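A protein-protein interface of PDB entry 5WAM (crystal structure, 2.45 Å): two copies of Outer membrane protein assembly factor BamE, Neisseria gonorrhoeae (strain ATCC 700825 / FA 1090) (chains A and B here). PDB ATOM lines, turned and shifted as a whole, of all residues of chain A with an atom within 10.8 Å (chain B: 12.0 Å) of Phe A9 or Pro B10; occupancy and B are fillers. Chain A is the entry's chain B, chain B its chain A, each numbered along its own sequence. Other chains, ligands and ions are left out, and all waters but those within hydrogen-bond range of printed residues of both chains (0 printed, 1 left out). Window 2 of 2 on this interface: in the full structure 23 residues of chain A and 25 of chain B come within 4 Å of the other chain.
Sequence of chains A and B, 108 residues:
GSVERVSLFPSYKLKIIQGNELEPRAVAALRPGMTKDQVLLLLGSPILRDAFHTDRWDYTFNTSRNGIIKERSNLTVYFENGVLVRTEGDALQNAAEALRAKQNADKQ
The side-chain hydroxyl (OG) of Ser A7 sits at hydrogen-bond distance from the backbone carbonyl oxygen (O) of Phe A9 (3.1 Å).
Phe A9 touches Pro B10, and with the chains exchanged Pro A10 touches Phe B9. Phe A9 touches Ser B11, but with the chains exchanged Ser A11 does not touch Phe B9 (7.7 Å). Pro A10 touches Ser B11, but with the chains exchanged Ser A11 does not touch Pro B10 (11.0 Å). Pro A10 touches Tyr B12, but with the chains exchanged Tyr A12 does not touch Pro B10 (9.9 Å). Positions printed for both chains: 7, 8, 9, 10, 11 and 12.
N of Lys B13 sits at hydrogen-bond distance from O of Pro A10, at 3.0 Å. The backbone carbonyl oxygen of Lys B13 sits at hydrogen-bond distance from the backbone NH of Tyr A12 (3.0 Å). The backbone carbonyl oxygen (O) of Tyr A12 lies within hydrogen-bond range of the backbone NH (N) of Lys B15 (3.0 Å).
Pro B10 touches Phe A9 (CD to CE1, 3.6 Å). Ser B11 touches Phe A9. Phe B9 touches Pro A10 (CD1 to CD, 3.7 Å). Pro A10 touches Ser B11 (CD to O, 3.8 Å). Tyr B12 touches Pro A10. Ser A11 touches Lys B13 (CA to O, 3.3 Å). O of Tyr A12 touches CA of Leu B14, at 3.5 Å.
Of chain B, only Pro B10 and Ser B11 come within 4 Å of Phe A9. No residue of chain B comes within 4 Å of Ser A7. No residue of chain B comes within 4 Å of Leu A8. Printed residues of chain B within 4 Å of Pro A10: Phe B9 (3.7 Å), Ser B11 (3.8 Å), Tyr B12 (3.5 Å) and Lys B13 (3.0 Å). Phe B9 touches one residue of chain A. Of the printed residues of chain A, Tyr B12 touches Pro A10 (3.5 Å). Printed residues of chain A within 4 Å of Lys B13: Pro A10, Ser A11 and Tyr A12. Of the printed residues of chain A, Lys B15 touches Tyr A12 (3.0 Å). Of the printed residues of chain B, Tyr A12 touches Lys B13 (3.0 Å), Leu B14 (3.5 Å) and Lys B15 (3.0 Å). Leu B8 touches none of the printed residues of chain A. Ser B7 touches none of the printed residues of chain A. The nearest printed residue of chain A that does not touch Leu B14 is Ser A11 (4.9 Å).
Hydrophobic or aromatic side chains of chain B within 4 Å of the printed part of chain A: Phe B9, Pro B10, Tyr B12 and Leu B14. Printed residues of chain A that touch a printed residue of chain B: Phe A9, Pro A10, Ser A11 and Tyr A12. Along chain A the printed residues that touch a printed residue of chain B span positions 9 to 12.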
ATOM      1  N   SER A   7       2.156   2.698 -18.118  1.00  0.00           N
ATOM      2  CA  SER A   7       1.774   1.292 -18.142  1.00  0.00           C
ATOM      3  C   SER A   7       2.781   0.445 -17.366  1.00  0.00           C
ATOM      4  O   SER A   7       3.990   0.627 -17.502  1.00  0.00           O
ATOM      5  CB  SER A   7       1.663   0.794 -19.585  1.00  0.00           C
ATOM      6  OG  SER A   7       1.163  -0.532 -19.637  1.00  0.00           O
ATOM      7  N   LEU A   8       2.275  -0.481 -16.547  1.00  0.00           N
ATOM      8  CA  LEU A   8       3.143  -1.365 -15.779  1.00  0.00           C
ATOM      9  C   LEU A   8       3.769  -2.455 -16.634  1.00  0.00           C
ATOM     10  O   LEU A   8       4.814  -2.997 -16.257  1.00  0.00           O
ATOM     11  CB  LEU A   8       2.356  -2.022 -14.640  1.00  0.00           C
ATOM     12  CG  LEU A   8       3.171  -2.791 -13.596  1.00  0.00           C
ATOM     13  CD1 LEU A   8       4.011  -1.852 -12.743  1.00  0.00           C
ATOM     14  CD2 LEU A   8       2.254  -3.632 -12.725  1.00  0.00           C
ATOM     15  N   PHE A   9       3.153  -2.792 -17.765  1.00  0.00           N
ATOM     16  CA  PHE A   9       3.609  -3.874 -18.616  1.00  0.00           C
ATOM     17  C   PHE A   9       4.081  -3.343 -19.964  1.00  0.00           C
ATOM     18  O   PHE A   9       3.397  -2.512 -20.573  1.00  0.00           O
ATOM     19  CB  PHE A   9       2.483  -4.888 -18.840  1.00  0.00           C
ATOM     20  CG  PHE A   9       1.993  -5.542 -17.575  1.00  0.00           C
ATOM     21  CD1 PHE A   9       2.851  -5.749 -16.504  1.00  0.00           C
ATOM     22  CD2 PHE A   9       0.673  -5.943 -17.454  1.00  0.00           C
ATOM     23  CE1 PHE A   9       2.403  -6.347 -15.342  1.00  0.00           C
ATOM     24  CE2 PHE A   9       0.221  -6.542 -16.293  1.00  0.00           C
ATOM     25  CZ  PHE A   9       1.089  -6.744 -15.236  1.00  0.00           C
ATOM     26  N   PRO A  10       5.224  -3.800 -20.461  1.00  0.00           N
ATOM     27  CA  PRO A  10       5.736  -3.285 -21.732  1.00  0.00           C
ATOM     28  C   PRO A  10       4.935  -3.823 -22.909  1.00  0.00           C
ATOM     29  O   PRO A  10       4.078  -4.698 -22.776  1.00  0.00           O
ATOM     30  CB  PRO A  10       7.177  -3.796 -21.760  1.00  0.00           C
ATOM     31  CG  PRO A  10       7.117  -5.074 -21.013  1.00  0.00           C
ATOM     32  CD  PRO A  10       6.071  -4.889 -19.938  1.00  0.00           C
ATOM     33  N   SER A  11       5.238  -3.276 -24.082  1.00  0.00           N
ATOM     34  CA  SER A  11       4.555  -3.640 -25.314  1.00  0.00           C
ATOM     35  C   SER A  11       5.573  -3.620 -26.442  1.00  0.00           C
ATOM     36  O   SER A  11       6.327  -2.654 -26.579  1.00  0.00           O
ATOM     37  CB  SER A  11       3.399  -2.679 -25.608  1.00  0.00           C
ATOM     38  OG  SER A  11       2.586  -3.161 -26.664  1.00  0.00           O
ATOM     39  N   TYR A  12       5.597  -4.687 -27.239  1.00  0.00           N
ATOM     40  CA  TYR A  12       6.585  -4.846 -28.293  1.00  0.00           C
ATOM     41  C   TYR A  12       5.897  -5.215 -29.598  1.00  0.00           C
ATOM     42  O   TYR A  12       4.794  -5.768 -29.614  1.00  0.00           O
ATOM     43  CB  TYR A  12       7.616  -5.924 -27.939  1.00  0.00           C
ATOM     44  CG  TYR A  12       8.195  -5.787 -26.552  1.00  0.00           C
ATOM     45  CD1 TYR A  12       7.587  -6.399 -25.464  1.00  0.00           C
ATOM     46  CD2 TYR A  12       9.350  -5.048 -26.328  1.00  0.00           C
ATOM     47  CE1 TYR A  12       8.113  -6.280 -24.191  1.00  0.00           C
ATOM     48  CE2 TYR A  12       9.884  -4.923 -25.060  1.00  0.00           C
ATOM     49  CZ  TYR A  12       9.262  -5.540 -23.995  1.00  0.00           C
ATOM     50  OH  TYR A  12       9.788  -5.418 -22.728  1.00  0.00           O
ATOM     51  N   VAL B   6      15.008 -14.781 -10.522  1.00  0.00           N
ATOM     52  CA  VAL B   6      14.982 -13.978 -11.737  1.00  0.00           C
ATOM     53  C   VAL B   6      13.734 -13.102 -11.744  1.00  0.00           C
ATOM     54  O   VAL B   6      12.643 -13.558 -11.398  1.00  0.00           O
ATOM     55  CB  VAL B   6      15.044 -14.870 -12.998  1.00  0.00           C
ATOM     56  CG1 VAL B   6      13.802 -15.747 -13.110  1.00  0.00           C
ATOM     57  CG2 VAL B   6      15.229 -14.021 -14.250  1.00  0.00           C
ATOM     58  N   SER B   7      13.900 -11.844 -12.143  1.00  0.00           N
ATOM     59  CA  SER B   7      12.799 -10.890 -12.182  1.00  0.00           C
ATOM     60  C   SER B   7      12.144 -10.924 -13.557  1.00  0.00           C
ATOM     61  O   SER B   7      12.821 -10.774 -14.579  1.00  0.00           O
ATOM     62  CB  SER B   7      13.301  -9.482 -11.863  1.00  0.00           C
ATOM     63  OG  SER B   7      12.251  -8.533 -11.937  1.00  0.00           O
ATOM     64  N   LEU B   8      10.827 -11.123 -13.578  1.00  0.00           N
ATOM     65  CA  LEU B   8      10.070 -11.225 -14.816  1.00  0.00           C
ATOM     66  C   LEU B   8       8.885 -10.274 -14.786  1.00  0.00           C
ATOM     67  O   LEU B   8       8.287 -10.032 -13.733  1.00  0.00           O
ATOM     68  CB  LEU B   8       9.554 -12.654 -15.049  1.00  0.00           C
ATOM     69  CG  LEU B   8      10.580 -13.743 -15.352  1.00  0.00           C
ATOM     70  CD1 LEU B   8       9.875 -15.079 -15.524  1.00  0.00           C
ATOM     71  CD2 LEU B   8      11.392 -13.403 -16.593  1.00  0.00           C
ATOM     72  N   PHE B   9       8.546  -9.742 -15.954  1.00  0.00           N
ATOM     73  CA  PHE B   9       7.294  -9.018 -16.096  1.00  0.00           C
ATOM     74  C   PHE B   9       6.134  -9.985 -15.883  1.00  0.00           C
ATOM     75  O   PHE B   9       6.110 -11.057 -16.504  1.00  0.00           O
ATOM     76  CB  PHE B   9       7.188  -8.375 -17.480  1.00  0.00           C
ATOM     77  CG  PHE B   9       8.108  -7.204 -17.683  1.00  0.00           C
ATOM     78  CD1 PHE B   9       7.914  -6.024 -16.985  1.00  0.00           C
ATOM     79  CD2 PHE B   9       9.156  -7.279 -18.583  1.00  0.00           C
ATOM     80  CE1 PHE B   9       8.757  -4.946 -17.173  1.00  0.00           C
ATOM     81  CE2 PHE B   9      10.000  -6.205 -18.775  1.00  0.00           C
ATOM     82  CZ  PHE B   9       9.801  -5.036 -18.070  1.00  0.00           C
ATOM     83  N   PRO B  10       5.167  -9.667 -15.019  1.00  0.00           N
ATOM     84  CA  PRO B  10       4.010 -10.567 -14.884  1.00  0.00           C
ATOM     85  C   PRO B  10       3.239 -10.717 -16.177  1.00  0.00           C
ATOM     86  O   PRO B  10       2.569 -11.736 -16.384  1.00  0.00           O
ATOM     87  CB  PRO B  10       3.159  -9.897 -13.795  1.00  0.00           C
ATOM     88  CG  PRO B  10       4.080  -8.956 -13.097  1.00  0.00           C
ATOM     89  CD  PRO B  10       5.062  -8.503 -14.125  1.00  0.00           C
ATOM     90  N   SER B  11       3.322  -9.726 -17.057  1.00  0.00           N
ATOM     91  CA  SER B  11       2.617  -9.762 -18.326  1.00  0.00           C
ATOM     92  C   SER B  11       3.207  -8.696 -19.235  1.00  0.00           C
ATOM     93  O   SER B  11       3.722  -7.680 -18.764  1.00  0.00           O
ATOM     94  CB  SER B  11       1.115  -9.531 -18.133  1.00  0.00           C
ATOM     95  OG  SER B  11       0.429  -9.545 -19.370  1.00  0.00           O
ATOM     96  N   TYR B  12       3.141  -8.950 -20.538  1.00  0.00           N
ATOM     97  CA  TYR B  12       3.515  -7.950 -21.525  1.00  0.00           C
ATOM     98  C   TYR B  12       2.664  -8.160 -22.766  1.00  0.00           C
ATOM     99  O   TYR B  12       2.088  -9.230 -22.975  1.00  0.00           O
ATOM    100  CB  TYR B  12       5.011  -8.011 -21.865  1.00  0.00           C
ATOM    101  CG  TYR B  12       5.475  -9.317 -22.473  1.00  0.00           C
ATOM    102  CD1 TYR B  12       5.931 -10.354 -21.673  1.00  0.00           C
ATOM    103  CD2 TYR B  12       5.474  -9.505 -23.849  1.00  0.00           C
ATOM    104  CE1 TYR B  12       6.362 -11.548 -22.224  1.00  0.00           C
ATOM    105  CE2 TYR B  12       5.905 -10.695 -24.410  1.00  0.00           C
ATOM    106  CZ  TYR B  12       6.349 -11.712 -23.592  1.00  0.00           C
ATOM    107  OH  TYR B  12       6.777 -12.897 -24.147  1.00  0.00           O
ATOM    108  N   LYS B  13       2.578  -7.115 -23.581  1.00  0.00           N
ATOM    109  CA  LYS B  13       1.774  -7.137 -24.791  1.00  0.00           C
ATOM    110  C   LYS B  13       2.666  -7.298 -26.014  1.00  0.00           C
ATOM    111  O   LYS B  13       3.791  -6.794 -26.060  1.00  0.00           O
ATOM    112  CB  LYS B  13       0.941  -5.862 -24.915  1.00  0.00           C
ATOM    113  CG  LYS B  13      -0.312  -5.867 -24.056  1.00  0.00           C
ATOM    114  CD  LYS B  13      -1.010  -4.515 -24.067  1.00  0.00           C
ATOM    115  CE  LYS B  13      -1.493  -4.138 -25.461  1.00  0.00           C
ATOM    116  NZ  LYS B  13      -2.195  -2.825 -25.471  1.00  0.00           N
ATOM    117  N   LEU B  14       2.146  -8.008 -27.011  1.00  0.00           N
ATOM    118  CA  LEU B  14       2.924  -8.367 -28.189  1.00  0.00           C
ATOM    119  C   LEU B  14       2.035  -8.266 -29.416  1.00  0.00           C
ATOM    120  O   LEU B  14       1.017  -8.959 -29.506  1.00  0.00           O
ATOM    121  CB  LEU B  14       3.492  -9.782 -28.042  1.00  0.00           C
ATOM    122  CG  LEU B  14       4.687 -10.186 -28.901  1.00  0.00           C
ATOM    123  CD1 LEU B  14       5.875  -9.271 -28.660  1.00  0.00           C
ATOM    124  CD2 LEU B  14       5.059 -11.628 -28.594  1.00  0.00           C
ATOM    125  N   LYS B  15       2.409  -7.397 -30.350  1.00  0.00           N
ATOM    126  CA  LYS B  15       1.748  -7.305 -31.646  1.00  0.00           C
ATOM    127  C   LYS B  15       2.618  -8.016 -32.673  1.00  0.00           C
ATOM    128  O   LYS B  15       3.795  -7.676 -32.836  1.00  0.00           O
ATOM    129  CB  LYS B  15       1.515  -5.851 -32.056  1.00  0.00           C
ATOM    130  CG  LYS B  15       0.726  -5.704 -33.349  1.00  0.00           C
ATOM    131  CD  LYS B  15       0.683  -4.263 -33.821  1.00  0.00           C
ATOM    132  CE  LYS B  15      -0.296  -4.084 -34.969  1.00  0.00           C
ATOM    133  NZ  LYS B  15       0.315  -3.361 -36.117  1.00  0.00           N
